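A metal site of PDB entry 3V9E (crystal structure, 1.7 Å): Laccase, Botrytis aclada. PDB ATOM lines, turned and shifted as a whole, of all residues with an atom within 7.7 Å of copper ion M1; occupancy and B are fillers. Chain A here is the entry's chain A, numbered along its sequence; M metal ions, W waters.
The backbone NH (N) of His 126 is in hydrogen-bond range of the backbone carbonyl oxygen (O) of Trp 166, 2.9 Å away. A ring nitrogen (NE2) of His 126 lies within hydrogen-bond range of a ring nitrogen (NE2) of His 466. NE2 of His 126 lies within hydrogen-bond range of OD1 of Asp 500, 2.9 Å away. The backbone carbonyl oxygen (O) of His 126 is in hydrogen-bond range of the side-chain hydroxyl (OG1) of Thr 165, at 2.5 Å. The guanidinium group (NH1) of Arg 310 sits close to a ring nitrogen (NE2) of His 126 (3.4 Å). The backbone NH (N) of His 124 sits at hydrogen-bond distance from the backbone carbonyl oxygen (O) of His 168 (2.8 Å). The backbone carbonyl oxygen (O) of His 527 lies within hydrogen-bond range of the side-chain hydroxyl (OH) of Tyr 175 (3.0 Å).
Residues that only touch copper ion M1: Trp 166 (3.3 Å). Within 4 Å of copper ion M1: His 126, Trp 166, His 168 and His 527.
A ring nitrogen (ND1) of His 126 is bound to copper ion M1 (1.8 Å). NE2 of His 168 binds copper ion M1, at 2.0 Å. NE2 of His 527 is bound to copper ion M1.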
ATOM      1  N   HIS A 124       7.783  13.140  -1.750  1.00  0.00           N
ATOM      2  CA  HIS A 124       6.555  13.166  -1.032  1.00  0.00           C
ATOM      3  C   HIS A 124       5.359  13.445  -1.969  1.00  0.00           C
ATOM      4  O   HIS A 124       5.508  14.160  -2.914  1.00  0.00           O
ATOM      5  CB  HIS A 124       6.637  14.270   0.012  1.00  0.00           C
ATOM      6  CG  HIS A 124       5.354  14.596   0.669  1.00  0.00           C
ATOM      7  ND1 HIS A 124       4.700  13.703   1.479  1.00  0.00           N
ATOM      8  CD2 HIS A 124       4.614  15.739   0.706  1.00  0.00           C
ATOM      9  CE1 HIS A 124       3.596  14.256   1.959  1.00  0.00           C
ATOM     10  NE2 HIS A 124       3.531  15.501   1.512  1.00  0.00           N
ATOM     11  N   TRP A 125       4.236  12.822  -1.622  1.00  0.00           N
ATOM     12  CA  TRP A 125       2.966  12.839  -2.413  1.00  0.00           C
ATOM     13  C   TRP A 125       2.081  13.748  -1.561  1.00  0.00           C
ATOM     14  O   TRP A 125       1.571  13.325  -0.534  1.00  0.00           O
ATOM     15  CB  TRP A 125       2.454  11.403  -2.643  1.00  0.00           C
ATOM     16  CG  TRP A 125       3.664  10.539  -2.878  1.00  0.00           C
ATOM     17  CD1 TRP A 125       4.345   9.824  -1.942  1.00  0.00           C
ATOM     18  CD2 TRP A 125       4.344  10.357  -4.105  1.00  0.00           C
ATOM     19  NE1 TRP A 125       5.427   9.204  -2.502  1.00  0.00           N
ATOM     20  CE2 TRP A 125       5.511   9.584  -3.814  1.00  0.00           C
ATOM     21  CE3 TRP A 125       4.147  10.833  -5.409  1.00  0.00           C
ATOM     22  CZ2 TRP A 125       6.415   9.249  -4.759  1.00  0.00           C
ATOM     23  CZ3 TRP A 125       5.108  10.538  -6.348  1.00  0.00           C
ATOM     24  CH2 TRP A 125       6.246   9.742  -6.036  1.00  0.00           C
ATOM     25  N   HIS A 126       2.005  15.026  -1.984  1.00  0.00           N
ATOM     26  CA  HIS A 126       1.550  16.054  -1.104  1.00  0.00           C
ATOM     27  C   HIS A 126       0.092  15.833  -0.781  1.00  0.00           C
ATOM     28  O   HIS A 126      -0.782  15.793  -1.655  1.00  0.00           O
ATOM     29  CB  HIS A 126       1.806  17.446  -1.671  1.00  0.00           C
ATOM     30  CG  HIS A 126       1.454  18.494  -0.700  1.00  0.00           C
ATOM     31  ND1 HIS A 126       2.380  19.302  -0.104  1.00  0.00           N
ATOM     32  CD2 HIS A 126       0.256  18.856  -0.205  1.00  0.00           C
ATOM     33  CE1 HIS A 126       1.773  20.145   0.691  1.00  0.00           C
ATOM     34  NE2 HIS A 126       0.490  19.868   0.685  1.00  0.00           N
ATOM     35  N   GLY A 127      -0.209  15.806   0.515  1.00  0.00           N
ATOM     36  CA  GLY A 127      -1.583  15.703   1.000  1.00  0.00           C
ATOM     37  C   GLY A 127      -2.094  14.317   1.011  1.00  0.00           C
ATOM     38  O   GLY A 127      -3.269  14.095   1.343  1.00  0.00           O
ATOM     39  N   THR A 165      -3.461  17.671  -6.478  1.00  0.00           N
ATOM     40  CA  THR A 165      -2.226  17.807  -5.647  1.00  0.00           C
ATOM     41  C   THR A 165      -0.976  17.745  -6.517  1.00  0.00           C
ATOM     42  O   THR A 165      -0.999  17.957  -7.717  1.00  0.00           O
ATOM     43  CB  THR A 165      -2.243  16.898  -4.399  1.00  0.00           C
ATOM     44  OG1 THR A 165      -1.294  17.441  -3.491  1.00  0.00           O
ATOM     45  CG2 THR A 165      -1.939  15.384  -4.744  1.00  0.00           C
ATOM     46  N   TRP A 166       0.158  17.567  -5.853  1.00  0.00           N
ATOM     47  CA  TRP A 166       1.424  17.577  -6.499  1.00  0.00           C
ATOM     48  C   TRP A 166       2.355  16.641  -5.728  1.00  0.00           C
ATOM     49  O   TRP A 166       2.033  16.288  -4.606  1.00  0.00           O
ATOM     50  CB  TRP A 166       1.994  18.976  -6.557  1.00  0.00           C
ATOM     51  CG  TRP A 166       2.207  19.749  -5.237  1.00  0.00           C
ATOM     52  CD1 TRP A 166       1.331  19.909  -4.203  1.00  0.00           C
ATOM     53  CD2 TRP A 166       3.396  20.442  -4.828  1.00  0.00           C
ATOM     54  NE1 TRP A 166       1.864  20.676  -3.195  1.00  0.00           N
ATOM     55  CE2 TRP A 166       3.107  21.077  -3.593  1.00  0.00           C
ATOM     56  CE3 TRP A 166       4.619  20.668  -5.418  1.00  0.00           C
ATOM     57  CZ2 TRP A 166       4.069  21.782  -2.874  1.00  0.00           C
ATOM     58  CZ3 TRP A 166       5.530  21.398  -4.771  1.00  0.00           C
ATOM     59  CH2 TRP A 166       5.293  21.953  -3.508  1.00  0.00           C
ATOM     60  N   TYR A 167       3.445  16.254  -6.360  1.00  0.00           N
ATOM     61  CA  TYR A 167       4.456  15.468  -5.727  1.00  0.00           C
ATOM     62  C   TYR A 167       5.743  16.223  -5.827  1.00  0.00           C
ATOM     63  O   TYR A 167       5.967  16.983  -6.778  1.00  0.00           O
ATOM     64  CB  TYR A 167       4.551  14.081  -6.331  1.00  0.00           C
ATOM     65  CG  TYR A 167       5.007  14.059  -7.755  1.00  0.00           C
ATOM     66  CD1 TYR A 167       4.119  14.310  -8.813  1.00  0.00           C
ATOM     67  CD2 TYR A 167       6.333  13.752  -8.084  1.00  0.00           C
ATOM     68  CE1 TYR A 167       4.555  14.216 -10.118  1.00  0.00           C
ATOM     69  CE2 TYR A 167       6.730  13.682  -9.387  1.00  0.00           C
ATOM     70  CZ  TYR A 167       5.855  13.982 -10.409  1.00  0.00           C
ATOM     71  OH  TYR A 167       6.340  13.894 -11.693  1.00  0.00           O
ATOM     72  N   HIS A 168       6.596  16.043  -4.843  1.00  0.00           N
ATOM     73  CA  HIS A 168       7.794  16.828  -4.850  1.00  0.00           C
ATOM     74  C   HIS A 168       8.804  16.260  -3.921  1.00  0.00           C
ATOM     75  O   HIS A 168       8.494  15.552  -2.970  1.00  0.00           O
ATOM     76  CB  HIS A 168       7.575  18.274  -4.463  1.00  0.00           C
ATOM     77  CG  HIS A 168       6.931  18.478  -3.122  1.00  0.00           C
ATOM     78  ND1 HIS A 168       7.659  18.587  -1.945  1.00  0.00           N
ATOM     79  CD2 HIS A 168       5.642  18.732  -2.787  1.00  0.00           C
ATOM     80  CE1 HIS A 168       6.833  18.831  -0.936  1.00  0.00           C
ATOM     81  NE2 HIS A 168       5.594  18.938  -1.418  1.00  0.00           N
ATOM     82  N   SER A 169      10.012  16.629  -4.189  1.00  0.00           N
ATOM     83  CA  SER A 169      11.043  16.244  -3.273  1.00  0.00           C
ATOM     84  C   SER A 169      10.816  16.882  -1.917  1.00  0.00           C
ATOM     85  O   SER A 169      10.443  18.027  -1.827  1.00  0.00           O
ATOM     86  CB  SER A 169      12.431  16.600  -3.748  1.00  0.00           C
ATOM     87  OG  SER A 169      13.363  16.284  -2.686  1.00  0.00           O
ATOM     88  N   HIS A 170      11.060  16.093  -0.854  1.00  0.00           N
ATOM     89  CA  HIS A 170      10.993  16.654   0.494  1.00  0.00           C
ATOM     90  C   HIS A 170      12.379  16.557   1.117  1.00  0.00           C
ATOM     91  O   HIS A 170      12.514  16.658   2.331  1.00  0.00           O
ATOM     92  CB  HIS A 170       9.996  15.847   1.318  1.00  0.00           C
ATOM     93  CG  HIS A 170       9.185  16.668   2.246  1.00  0.00           C
ATOM     94  ND1 HIS A 170       9.760  17.438   3.189  1.00  0.00           N
ATOM     95  CD2 HIS A 170       7.849  16.880   2.369  1.00  0.00           C
ATOM     96  CE1 HIS A 170       8.846  18.054   3.908  1.00  0.00           C
ATOM     97  NE2 HIS A 170       7.673  17.757   3.407  1.00  0.00           N
ATOM     98  N   TYR A 175      12.912  20.929  -4.198  1.00  0.00           N
ATOM     99  CA  TYR A 175      11.787  21.270  -5.014  1.00  0.00           C
ATOM    100  C   TYR A 175      11.894  22.655  -5.535  1.00  0.00           C
ATOM    101  O   TYR A 175      11.203  23.030  -6.528  1.00  0.00           O
ATOM    102  CB  TYR A 175      10.401  21.038  -4.321  1.00  0.00           C
ATOM    103  CG  TYR A 175       9.867  22.152  -3.456  1.00  0.00           C
ATOM    104  CD1 TYR A 175       9.068  23.098  -3.952  1.00  0.00           C
ATOM    105  CD2 TYR A 175      10.158  22.208  -2.088  1.00  0.00           C
ATOM    106  CE1 TYR A 175       8.555  24.116  -3.182  1.00  0.00           C
ATOM    107  CE2 TYR A 175       9.655  23.244  -1.274  1.00  0.00           C
ATOM    108  CZ  TYR A 175       8.822  24.200  -1.840  1.00  0.00           C
ATOM    109  OH  TYR A 175       8.286  25.267  -1.109  1.00  0.00           O
ATOM    110  N   ASN A 269       0.228  26.576  -5.644  1.00  0.00           N
ATOM    111  CA  ASN A 269       1.355  27.451  -5.369  1.00  0.00           C
ATOM    112  C   ASN A 269       2.513  26.528  -4.892  1.00  0.00           C
ATOM    113  O   ASN A 269       2.349  25.851  -3.909  1.00  0.00           O
ATOM    114  CB  ASN A 269       1.020  28.501  -4.307  1.00  0.00           C
ATOM    115  CG  ASN A 269       2.215  29.302  -3.805  1.00  0.00           C
ATOM    116  OD1 ASN A 269       3.368  29.065  -4.153  1.00  0.00           O
ATOM    117  ND2 ASN A 269       1.913  30.274  -2.926  1.00  0.00           N
ATOM    118  N   VAL A 270       3.583  26.524  -5.647  1.00  0.00           N
ATOM    119  CA  VAL A 270       4.732  25.627  -5.439  1.00  0.00           C
ATOM    120  C   VAL A 270       6.050  26.394  -5.314  1.00  0.00           C
ATOM    121  O   VAL A 270       7.121  25.800  -5.495  1.00  0.00           O
ATOM    122  CB  VAL A 270       4.823  24.486  -6.537  1.00  0.00           C
ATOM    123  CG1 VAL A 270       3.514  23.726  -6.521  1.00  0.00           C
ATOM    124  CG2 VAL A 270       5.154  25.060  -7.922  1.00  0.00           C
ATOM    125  N   ILE A 307       1.733  28.605  -0.068  1.00  0.00           N
ATOM    126  CA  ILE A 307       2.607  27.584  -0.622  1.00  0.00           C
ATOM    127  C   ILE A 307       2.123  26.180  -0.221  1.00  0.00           C
ATOM    128  O   ILE A 307       1.947  25.863   0.961  1.00  0.00           O
ATOM    129  CB  ILE A 307       4.052  27.718  -0.133  1.00  0.00           C
ATOM    130  CG1 ILE A 307       4.659  29.021  -0.631  1.00  0.00           C
ATOM    131  CG2 ILE A 307       4.858  26.556  -0.719  1.00  0.00           C
ATOM    132  CD1 ILE A 307       5.957  29.261   0.063  1.00  0.00           C
ATOM    133  N   GLY A 308       1.916  25.336  -1.196  1.00  0.00           N
ATOM    134  CA  GLY A 308       1.430  24.017  -0.933  1.00  0.00           C
ATOM    135  C   GLY A 308      -0.055  23.866  -1.009  1.00  0.00           C
ATOM    136  O   GLY A 308      -0.543  22.721  -1.122  1.00  0.00           O
ATOM    137  N   GLN A 309      -0.786  24.958  -0.929  1.00  0.00           N
ATOM    138  CA  GLN A 309      -2.173  24.962  -1.131  1.00  0.00           C
ATOM    139  C   GLN A 309      -2.545  24.726  -2.560  1.00  0.00           C
ATOM    140  O   GLN A 309      -1.837  25.102  -3.474  1.00  0.00           O
ATOM    141  CB  GLN A 309      -2.781  26.253  -0.738  1.00  0.00           C
ATOM    142  CG  GLN A 309      -2.634  26.428   0.737  1.00  0.00           C
ATOM    143  CD  GLN A 309      -3.485  27.583   1.264  1.00  0.00           C
ATOM    144  OE1 GLN A 309      -3.541  28.614   0.685  1.00  0.00           O
ATOM    145  NE2 GLN A 309      -4.080  27.378   2.441  1.00  0.00           N
ATOM    146  N   ARG A 310      -3.699  24.099  -2.738  1.00  0.00           N
ATOM    147  CA  ARG A 310      -4.299  23.884  -4.025  1.00  0.00           C
ATOM    148  C   ARG A 310      -5.715  24.353  -3.911  1.00  0.00           C
ATOM    149  O   ARG A 310      -6.289  24.298  -2.846  1.00  0.00           O
ATOM    150  CB  ARG A 310      -4.366  22.429  -4.521  1.00  0.00           C
ATOM    151  CG  ARG A 310      -3.009  21.804  -4.776  1.00  0.00           C
ATOM    152  CD  ARG A 310      -2.377  21.335  -3.491  1.00  0.00           C
ATOM    153  NE  ARG A 310      -3.035  20.153  -2.917  1.00  0.00           N
ATOM    154  CZ  ARG A 310      -3.072  19.864  -1.642  1.00  0.00           C
ATOM    155  NH1 ARG A 310      -2.503  20.606  -0.731  1.00  0.00           N
ATOM    156  NH2 ARG A 310      -3.602  18.692  -1.269  1.00  0.00           N
ATOM    157  N   HIS A 466       1.925  22.816   6.706  1.00  0.00           N
ATOM    158  CA  HIS A 466       1.532  21.554   6.085  1.00  0.00           C
ATOM    159  C   HIS A 466       1.575  20.449   7.127  1.00  0.00           C
ATOM    160  O   HIS A 466       2.571  20.291   7.755  1.00  0.00           O
ATOM    161  CB  HIS A 466       2.493  21.230   4.944  1.00  0.00           C
ATOM    162  CG  HIS A 466       2.210  19.929   4.278  1.00  0.00           C
ATOM    163  ND1 HIS A 466       3.192  19.105   3.736  1.00  0.00           N
ATOM    164  CD2 HIS A 466       1.027  19.290   4.103  1.00  0.00           C
ATOM    165  CE1 HIS A 466       2.613  18.025   3.258  1.00  0.00           C
ATOM    166  NE2 HIS A 466       1.314  18.124   3.445  1.00  0.00           N
ATOM    167  N   HIS A 468       1.287  16.298   7.459  1.00  0.00           N
ATOM    168  CA  HIS A 468       1.344  15.037   6.731  1.00  0.00           C
ATOM    169  C   HIS A 468       0.339  14.036   7.373  1.00  0.00           C
ATOM    170  O   HIS A 468       0.019  14.102   8.578  1.00  0.00           O
ATOM    171  CB  HIS A 468       2.777  14.510   6.767  1.00  0.00           C
ATOM    172  CG  HIS A 468       3.722  15.282   5.930  1.00  0.00           C
ATOM    173  ND1 HIS A 468       4.540  14.675   4.997  1.00  0.00           N
ATOM    174  CD2 HIS A 468       4.017  16.588   5.880  1.00  0.00           C
ATOM    175  CE1 HIS A 468       5.234  15.603   4.353  1.00  0.00           C
ATOM    176  NE2 HIS A 468       4.941  16.780   4.880  1.00  0.00           N
ATOM    177  N   ASP A 500      -5.081  20.448   3.978  1.00  0.00           N
ATOM    178  CA  ASP A 500      -3.764  20.001   4.487  1.00  0.00           C
ATOM    179  C   ASP A 500      -2.676  21.003   4.560  1.00  0.00           C
ATOM    180  O   ASP A 500      -1.584  20.735   5.146  1.00  0.00           O
ATOM    181  CB  ASP A 500      -3.305  18.715   3.738  1.00  0.00           C
ATOM    182  CG  ASP A 500      -3.078  18.944   2.273  1.00  0.00           C
ATOM    183  OD1 ASP A 500      -2.172  19.736   1.924  1.00  0.00           O
ATOM    184  OD2 ASP A 500      -3.805  18.323   1.450  1.00  0.00           O
ATOM    185  N   VAL A 501      -2.928  22.186   4.022  1.00  0.00           N
ATOM    186  CA  VAL A 501      -1.970  23.326   4.210  1.00  0.00           C
ATOM    187  C   VAL A 501      -2.822  24.521   4.614  1.00  0.00           C
ATOM    188  O   VAL A 501      -3.836  24.869   3.966  1.00  0.00           O
ATOM    189  CB  VAL A 501      -1.159  23.667   2.960  1.00  0.00           C
ATOM    190  CG1 VAL A 501      -0.326  24.942   3.171  1.00  0.00           C
ATOM    191  CG2 VAL A 501      -0.260  22.512   2.582  1.00  0.00           C
ATOM    192  N   HIS A 525       5.080  21.221   9.265  1.00  0.00           N
ATOM    193  CA  HIS A 525       6.067  22.201   8.983  1.00  0.00           C
ATOM    194  C   HIS A 525       5.575  23.325   8.166  1.00  0.00           C
ATOM    195  O   HIS A 525       4.592  23.217   7.433  1.00  0.00           O
ATOM    196  CB  HIS A 525       7.246  21.540   8.251  1.00  0.00           C
ATOM    197  CG  HIS A 525       6.872  21.015   6.891  1.00  0.00           C
ATOM    198  ND1 HIS A 525       7.197  21.721   5.749  1.00  0.00           N
ATOM    199  CD2 HIS A 525       6.214  19.904   6.490  1.00  0.00           C
ATOM    200  CE1 HIS A 525       6.767  21.025   4.691  1.00  0.00           C
ATOM    201  NE2 HIS A 525       6.156  19.929   5.121  1.00  0.00           N
ATOM    202  N   HIS A 527       5.902  25.506   4.957  1.00  0.00           N
ATOM    203  CA  HIS A 527       6.225  25.071   3.567  1.00  0.00           C
ATOM    204  C   HIS A 527       7.028  26.128   2.856  1.00  0.00           C
ATOM    205  O   HIS A 527       7.382  25.921   1.723  1.00  0.00           O
ATOM    206  CB  HIS A 527       4.918  24.747   2.780  1.00  0.00           C
ATOM    207  CG  HIS A 527       5.030  23.606   1.814  1.00  0.00           C
ATOM    208  ND1 HIS A 527       5.935  23.589   0.774  1.00  0.00           N
ATOM    209  CD2 HIS A 527       4.299  22.454   1.699  1.00  0.00           C
ATOM    210  CE1 HIS A 527       5.770  22.492   0.051  1.00  0.00           C
ATOM    211  NE2 HIS A 527       4.785  21.770   0.601  1.00  0.00           N
HETATM  212 CU    CU M   1       4.159  19.707  -0.261  1.00  0.00          CU
HETATM  213 CU    CU M   2       5.693  18.368   4.019  1.00  0.00          CU
HETATM  214  O   HOH W   1       5.710  19.191   2.167  1.00  0.00           O
